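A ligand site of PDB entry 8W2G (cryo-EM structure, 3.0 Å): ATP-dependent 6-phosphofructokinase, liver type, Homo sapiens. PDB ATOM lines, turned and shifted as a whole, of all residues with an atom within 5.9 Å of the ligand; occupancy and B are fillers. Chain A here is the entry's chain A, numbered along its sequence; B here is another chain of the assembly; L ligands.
OE2 of Glu 628 sits at hydrogen-bond distance from O6 of the ligand.
OG1 of Thr 527 sits at hydrogen-bond distance from O11 of the ligand, 2.6 Å away.
An oxygen (O10) of the ligand is in salt-bridge range of the guanidinium group of Arg 470 (2.7 Å).
The guanidinium group of Arg 654 of chain B is in salt-bridge range of an oxygen (O3) of the ligand (2.7 Å).
An oxygen (O10) of the ligand lies within salt-bridge range of the guanidinium group of Arg 734 (2.8 Å).
An oxygen (O7) of the ligand is in hydrogen-bond range of the side-chain sulfur of Met 572 (2.8 Å).
NH1 of Arg 565 of chain B is in salt-bridge range of O2 of the ligand (3.0 Å).
O12 of the ligand lies close to OG of Ser 529, 3.4 Å away.
N of Gly 573 sits at hydrogen-bond distance from O6 of the ligand, 3.2 Å away.
The side-chain amide oxygen (OD1) of Asn 531 sits close to an oxygen (O11) of the ligand.
NE2 of His 660 lies within hydrogen-bond range of O3 of the ligand, 3.4 Å away.
Ala 409 touches the ligand.
Ile 528 touches the ligand (CD1 to O7, 3.7 Å).
Gly 574 touches the ligand.
Gln 663 touches the ligand (NE2 to O7, 3.5 Å).
Hydrophobic or aromatic side chains that line the ligand: Ala 409, Ile 528 and Met 572.
15 residues have an atom within 4 Å of the ligand: Ala 409, Arg 470, Thr 527, Ile 528, Ser 529, Asn 531, Met 572, Gly 573, Gly 574, Glu 628, His 660, Gln 663, Arg 734, Arg 565 of chain B and Arg 654 of chain B.
The side-chain carboxylate (OE2) of Glu 628 is in hydrogen-bond range of the backbone NH (N) of Gly 573, at 3.0 Å.
OE2 of Glu 628 lies within hydrogen-bond range of N of Gly 574 (2.8 Å).
The side-chain amide nitrogen of Asn 531 sits at hydrogen-bond distance from the backbone carbonyl oxygen of Arg 734 (3.2 Å).
NE of Arg 734 is in salt-bridge range of OE1 of Glu 499 (3.8 Å).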
ATOM      1  N   GLY A 408      -8.325  27.865  11.892  1.00  0.00           N
ATOM      2  CA  GLY A 408      -8.363  26.561  12.525  1.00  0.00           C
ATOM      3  C   GLY A 408      -9.112  26.608  13.841  1.00  0.00           C
ATOM      4  O   GLY A 408      -9.898  27.526  14.114  1.00  0.00           O
ATOM      5  N   ALA A 409      -8.872  25.598  14.666  1.00  0.00           N
ATOM      6  CA  ALA A 409      -9.451  25.570  15.997  1.00  0.00           C
ATOM      7  C   ALA A 409      -8.624  26.459  16.935  1.00  0.00           C
ATOM      8  O   ALA A 409      -7.427  26.653  16.720  1.00  0.00           O
ATOM      9  CB  ALA A 409      -9.481  24.151  16.542  1.00  0.00           C
ATOM     10  N   ARG A 470     -12.568  27.641  10.505  1.00  0.00           N
ATOM     11  CA  ARG A 470     -12.008  26.614   9.620  1.00  0.00           C
ATOM     12  C   ARG A 470     -12.180  26.945   8.144  1.00  0.00           C
ATOM     13  O   ARG A 470     -11.759  26.143   7.296  1.00  0.00           O
ATOM     14  CB  ARG A 470     -12.659  25.252   9.894  1.00  0.00           C
ATOM     15  CG  ARG A 470     -12.912  24.884  11.364  1.00  0.00           C
ATOM     16  CD  ARG A 470     -11.633  24.790  12.194  1.00  0.00           C
ATOM     17  NE  ARG A 470     -10.949  23.518  12.015  1.00  0.00           N
ATOM     18  CZ  ARG A 470     -10.920  22.504  12.874  1.00  0.00           C
ATOM     19  NH1 ARG A 470     -11.560  22.530  14.028  1.00  0.00           N
ATOM     20  NH2 ARG A 470     -10.225  21.407  12.553  1.00  0.00           N
ATOM     21  N   GLY A 497      -3.687  26.285  12.542  1.00  0.00           N
ATOM     22  CA  GLY A 497      -3.369  24.880  12.353  1.00  0.00           C
ATOM     23  C   GLY A 497      -3.219  24.487  10.900  1.00  0.00           C
ATOM     24  O   GLY A 497      -2.713  25.258  10.078  1.00  0.00           O
ATOM     25  N   PHE A 498      -3.647  23.266  10.585  1.00  0.00           N
ATOM     26  CA  PHE A 498      -3.513  22.763   9.217  1.00  0.00           C
ATOM     27  C   PHE A 498      -4.324  23.588   8.227  1.00  0.00           C
ATOM     28  O   PHE A 498      -3.930  23.743   7.070  1.00  0.00           O
ATOM     29  CB  PHE A 498      -3.953  21.298   9.145  1.00  0.00           C
ATOM     30  CG  PHE A 498      -3.514  20.598   7.889  1.00  0.00           C
ATOM     31  CD1 PHE A 498      -4.298  20.606   6.747  1.00  0.00           C
ATOM     32  CD2 PHE A 498      -2.307  19.915   7.853  1.00  0.00           C
ATOM     33  CE1 PHE A 498      -3.889  19.974   5.595  1.00  0.00           C
ATOM     34  CE2 PHE A 498      -1.895  19.271   6.709  1.00  0.00           C
ATOM     35  CZ  PHE A 498      -2.681  19.305   5.579  1.00  0.00           C
ATOM     36  N   GLU A 499      -5.461  24.127   8.671  1.00  0.00           N
ATOM     37  CA  GLU A 499      -6.281  24.957   7.789  1.00  0.00           C
ATOM     38  C   GLU A 499      -5.543  26.224   7.379  1.00  0.00           C
ATOM     39  O   GLU A 499      -5.762  26.739   6.276  1.00  0.00           O
ATOM     40  CB  GLU A 499      -7.602  25.298   8.472  1.00  0.00           C
ATOM     41  CG  GLU A 499      -8.463  24.094   8.848  1.00  0.00           C
ATOM     42  CD  GLU A 499      -9.059  23.406   7.636  1.00  0.00           C
ATOM     43  OE1 GLU A 499      -8.331  22.668   6.943  1.00  0.00           O
ATOM     44  OE2 GLU A 499     -10.268  23.614   7.366  1.00  0.00           O
ATOM     45  N   THR A 527      -1.858  24.682  17.000  1.00  0.00           N
ATOM     46  CA  THR A 527      -2.950  23.730  17.134  1.00  0.00           C
ATOM     47  C   THR A 527      -2.568  22.700  18.194  1.00  0.00           C
ATOM     48  O   THR A 527      -1.387  22.399  18.392  1.00  0.00           O
ATOM     49  CB  THR A 527      -3.278  23.031  15.811  1.00  0.00           C
ATOM     50  OG1 THR A 527      -4.387  22.145  16.005  1.00  0.00           O
ATOM     51  CG2 THR A 527      -2.082  22.248  15.278  1.00  0.00           C
ATOM     52  N   ILE A 528      -3.588  22.162  18.862  1.00  0.00           N
ATOM     53  CA  ILE A 528      -3.343  21.183  19.912  1.00  0.00           C
ATOM     54  C   ILE A 528      -2.832  19.864  19.338  1.00  0.00           C
ATOM     55  O   ILE A 528      -2.096  19.122  19.999  1.00  0.00           O
ATOM     56  CB  ILE A 528      -4.612  20.972  20.770  1.00  0.00           C
ATOM     57  CG1 ILE A 528      -5.771  20.347  19.960  1.00  0.00           C
ATOM     58  CG2 ILE A 528      -5.054  22.300  21.385  1.00  0.00           C
ATOM     59  CD1 ILE A 528      -6.969  19.971  20.798  1.00  0.00           C
ATOM     60  N   SER A 529      -3.220  19.545  18.095  1.00  0.00           N
ATOM     61  CA  SER A 529      -2.986  18.215  17.543  1.00  0.00           C
ATOM     62  C   SER A 529      -1.553  17.989  17.099  1.00  0.00           C
ATOM     63  O   SER A 529      -1.142  16.832  16.957  1.00  0.00           O
ATOM     64  CB  SER A 529      -3.928  17.983  16.362  1.00  0.00           C
ATOM     65  OG  SER A 529      -5.249  18.382  16.680  1.00  0.00           O
ATOM     66  N   ASN A 530      -0.785  19.052  16.850  1.00  0.00           N
ATOM     67  CA  ASN A 530       0.607  18.937  16.414  1.00  0.00           C
ATOM     68  C   ASN A 530       0.692  18.225  15.053  1.00  0.00           C
ATOM     69  O   ASN A 530       1.483  17.296  14.853  1.00  0.00           O
ATOM     70  CB  ASN A 530       1.443  18.216  17.468  1.00  0.00           C
ATOM     71  CG  ASN A 530       2.910  18.588  17.406  1.00  0.00           C
ATOM     72  OD1 ASN A 530       3.252  19.773  17.414  1.00  0.00           O
ATOM     73  ND2 ASN A 530       3.776  17.592  17.347  1.00  0.00           N
ATOM     74  N   ASN A 531      -0.138  18.692  14.112  1.00  0.00           N
ATOM     75  CA  ASN A 531      -0.276  18.073  12.791  1.00  0.00           C
ATOM     76  C   ASN A 531       0.212  18.953  11.644  1.00  0.00           C
ATOM     77  O   ASN A 531       0.144  18.520  10.488  1.00  0.00           O
ATOM     78  CB  ASN A 531      -1.736  17.682  12.553  1.00  0.00           C
ATOM     79  CG  ASN A 531      -2.676  18.870  12.594  1.00  0.00           C
ATOM     80  OD1 ASN A 531      -2.507  19.766  13.414  1.00  0.00           O
ATOM     81  ND2 ASN A 531      -3.675  18.882  11.723  1.00  0.00           N
ATOM     82  N   MET A 572      -8.620  13.931  21.634  1.00  0.00           N
ATOM     83  CA  MET A 572      -8.722  14.650  20.372  1.00  0.00           C
ATOM     84  C   MET A 572      -7.389  14.565  19.624  1.00  0.00           C
ATOM     85  O   MET A 572      -6.405  14.013  20.125  1.00  0.00           O
ATOM     86  CB  MET A 572      -9.136  16.101  20.618  1.00  0.00           C
ATOM     87  CG  MET A 572     -10.580  16.250  21.094  1.00  0.00           C
ATOM     88  SD  MET A 572     -11.296  17.890  20.821  1.00  0.00           S
ATOM     89  CE  MET A 572     -10.261  18.916  21.861  1.00  0.00           C
ATOM     90  N   GLY A 573      -7.357  15.108  18.406  1.00  0.00           N
ATOM     91  CA  GLY A 573      -6.151  15.165  17.588  1.00  0.00           C
ATOM     92  C   GLY A 573      -6.321  14.708  16.146  1.00  0.00           C
ATOM     93  O   GLY A 573      -5.328  14.636  15.411  1.00  0.00           O
ATOM     94  N   GLY A 574      -7.542  14.417  15.723  1.00  0.00           N
ATOM     95  CA  GLY A 574      -7.755  13.933  14.369  1.00  0.00           C
ATOM     96  C   GLY A 574      -7.059  12.605  14.145  1.00  0.00           C
ATOM     97  O   GLY A 574      -7.151  11.684  14.974  1.00  0.00           O
ATOM     98  N   GLU A 628      -9.130   9.804  18.640  1.00  0.00           N
ATOM     99  CA  GLU A 628     -10.516   9.905  18.189  1.00  0.00           C
ATOM    100  C   GLU A 628     -10.743   9.312  16.798  1.00  0.00           C
ATOM    101  O   GLU A 628     -11.895   9.057  16.442  1.00  0.00           O
ATOM    102  CB  GLU A 628     -10.986  11.361  18.213  1.00  0.00           C
ATOM    103  CG  GLU A 628     -10.135  12.328  17.383  1.00  0.00           C
ATOM    104  CD  GLU A 628     -10.706  13.733  17.354  1.00  0.00           C
ATOM    105  OE1 GLU A 628     -11.888  13.905  17.743  1.00  0.00           O
ATOM    106  OE2 GLU A 628      -9.991  14.667  16.954  1.00  0.00           O
ATOM    107  N   HIS A 660     -13.587  19.108  24.399  1.00  0.00           N
ATOM    108  CA  HIS A 660     -12.843  20.352  24.227  1.00  0.00           C
ATOM    109  C   HIS A 660     -12.219  20.874  25.532  1.00  0.00           C
ATOM    110  O   HIS A 660     -11.762  22.015  25.566  1.00  0.00           O
ATOM    111  CB  HIS A 660     -13.754  21.408  23.605  1.00  0.00           C
ATOM    112  CG  HIS A 660     -14.381  20.978  22.319  1.00  0.00           C
ATOM    113  ND1 HIS A 660     -15.401  20.052  22.269  1.00  0.00           N
ATOM    114  CD2 HIS A 660     -14.128  21.330  21.037  1.00  0.00           C
ATOM    115  CE1 HIS A 660     -15.754  19.860  21.008  1.00  0.00           C
ATOM    116  NE2 HIS A 660     -14.999  20.617  20.235  1.00  0.00           N
ATOM    117  N   GLN A 663      -8.449  21.551  24.829  1.00  0.00           N
ATOM    118  CA  GLN A 663      -7.938  22.841  24.374  1.00  0.00           C
ATOM    119  C   GLN A 663      -7.379  23.672  25.525  1.00  0.00           C
ATOM    120  O   GLN A 663      -6.658  24.637  25.278  1.00  0.00           O
ATOM    121  CB  GLN A 663      -9.029  23.596  23.620  1.00  0.00           C
ATOM    122  CG  GLN A 663      -9.333  22.961  22.280  1.00  0.00           C
ATOM    123  CD  GLN A 663     -10.378  23.732  21.497  1.00  0.00           C
ATOM    124  OE1 GLN A 663     -10.813  24.795  21.925  1.00  0.00           O
ATOM    125  NE2 GLN A 663     -10.771  23.189  20.351  1.00  0.00           N
ATOM    126  N   ARG A 734      -4.526  15.094   6.886  1.00  0.00           N
ATOM    127  CA  ARG A 734      -4.139  16.397   7.442  1.00  0.00           C
ATOM    128  C   ARG A 734      -3.008  16.247   8.461  1.00  0.00           C
ATOM    129  O   ARG A 734      -3.151  16.554   9.643  1.00  0.00           O
ATOM    130  CB  ARG A 734      -5.347  17.115   8.048  1.00  0.00           C
ATOM    131  CG  ARG A 734      -6.427  17.461   7.015  1.00  0.00           C
ATOM    132  CD  ARG A 734      -7.746  17.873   7.647  1.00  0.00           C
ATOM    133  NE  ARG A 734      -7.681  19.164   8.323  1.00  0.00           N
ATOM    134  CZ  ARG A 734      -7.556  19.363   9.640  1.00  0.00           C
ATOM    135  NH1 ARG A 734      -7.465  18.366  10.504  1.00  0.00           N
ATOM    136  NH2 ARG A 734      -7.536  20.614  10.090  1.00  0.00           N
ATOM    137  N   THR B 562     -14.137  29.996  19.181  1.00  0.00           N
ATOM    138  CA  THR B 562     -14.881  29.607  17.977  1.00  0.00           C
ATOM    139  C   THR B 562     -16.262  30.251  18.075  1.00  0.00           C
ATOM    140  O   THR B 562     -17.222  29.622  18.509  1.00  0.00           O
ATOM    141  CB  THR B 562     -14.991  28.093  17.868  1.00  0.00           C
ATOM    142  OG1 THR B 562     -13.683  27.516  17.937  1.00  0.00           O
ATOM    143  CG2 THR B 562     -15.649  27.689  16.555  1.00  0.00           C
ATOM    144  N   ARG B 565     -21.030  29.363  18.770  1.00  0.00           N
ATOM    145  CA  ARG B 565     -21.028  27.961  19.144  1.00  0.00           C
ATOM    146  C   ARG B 565     -21.785  27.783  20.457  1.00  0.00           C
ATOM    147  O   ARG B 565     -21.771  28.658  21.321  1.00  0.00           O
ATOM    148  CB  ARG B 565     -19.605  27.408  19.296  1.00  0.00           C
ATOM    149  CG  ARG B 565     -19.561  25.949  19.749  1.00  0.00           C
ATOM    150  CD  ARG B 565     -18.263  25.258  19.387  1.00  0.00           C
ATOM    151  NE  ARG B 565     -18.123  25.059  17.950  1.00  0.00           N
ATOM    152  CZ  ARG B 565     -17.173  24.349  17.361  1.00  0.00           C
ATOM    153  NH1 ARG B 565     -16.224  23.735  18.060  1.00  0.00           N
ATOM    154  NH2 ARG B 565     -17.164  24.246  16.038  1.00  0.00           N
ATOM    155  N   ARG B 654     -22.001  21.487  19.776  1.00  0.00           N
ATOM    156  CA  ARG B 654     -21.122  20.390  20.141  1.00  0.00           C
ATOM    157  C   ARG B 654     -21.571  19.843  21.484  1.00  0.00           C
ATOM    158  O   ARG B 654     -22.325  20.502  22.211  1.00  0.00           O
ATOM    159  CB  ARG B 654     -19.645  20.839  20.221  1.00  0.00           C
ATOM    160  CG  ARG B 654     -19.029  21.240  18.895  1.00  0.00           C
ATOM    161  CD  ARG B 654     -18.778  20.039  17.996  1.00  0.00           C
ATOM    162  NE  ARG B 654     -18.155  20.418  16.736  1.00  0.00           N
ATOM    163  CZ  ARG B 654     -18.799  20.909  15.682  1.00  0.00           C
ATOM    164  NH1 ARG B 654     -20.103  21.121  15.696  1.00  0.00           N
ATOM    165  NH2 ARG B 654     -18.113  21.196  14.582  1.00  0.00           N
HETATM  166  P1  LIG L   1     -14.395  20.963  16.135  1.00  0.00           P
HETATM  167  O1  LIG L   1     -14.923  21.440  14.803  1.00  0.00           O
HETATM  168  O2  LIG L   1     -13.970  22.163  16.955  1.00  0.00           O
HETATM  169  O3  LIG L   1     -15.473  20.209  16.877  1.00  0.00           O
HETATM  170  O4  LIG L   1     -13.105  19.978  15.884  1.00  0.00           O
HETATM  171  C1  LIG L   1     -12.279  19.669  16.975  1.00  0.00           C
HETATM  172  C2  LIG L   1     -11.040  18.966  16.442  1.00  0.00           C
HETATM  173  O5  LIG L   1     -11.365  18.116  15.550  1.00  0.00           O
HETATM  174  C3  LIG L   1     -10.240  18.251  17.615  1.00  0.00           C
HETATM  175  O6  LIG L   1      -9.369  17.155  17.042  1.00  0.00           O
HETATM  176  C4  LIG L   1      -9.532  19.143  18.088  1.00  0.00           C
HETATM  177  O7  LIG L   1     -10.262  19.903  19.123  1.00  0.00           O
HETATM  178  C5  LIG L   1      -9.223  20.214  16.843  1.00  0.00           C
HETATM  179  O8  LIG L   1     -10.043  19.970  15.891  1.00  0.00           O
HETATM  180  C6  LIG L   1      -7.804  20.042  16.380  1.00  0.00           C
HETATM  181  O9  LIG L   1      -7.568  21.016  15.406  1.00  0.00           O
HETATM  182  P2  LIG L   1      -6.884  20.529  13.988  1.00  0.00           P
HETATM  183  O10 LIG L   1      -7.583  21.227  12.847  1.00  0.00           O
HETATM  184  O11 LIG L   1      -5.423  20.895  14.006  1.00  0.00           O
HETATM  185  O12 LIG L   1      -7.031  19.035  13.846  1.00  0.00           O
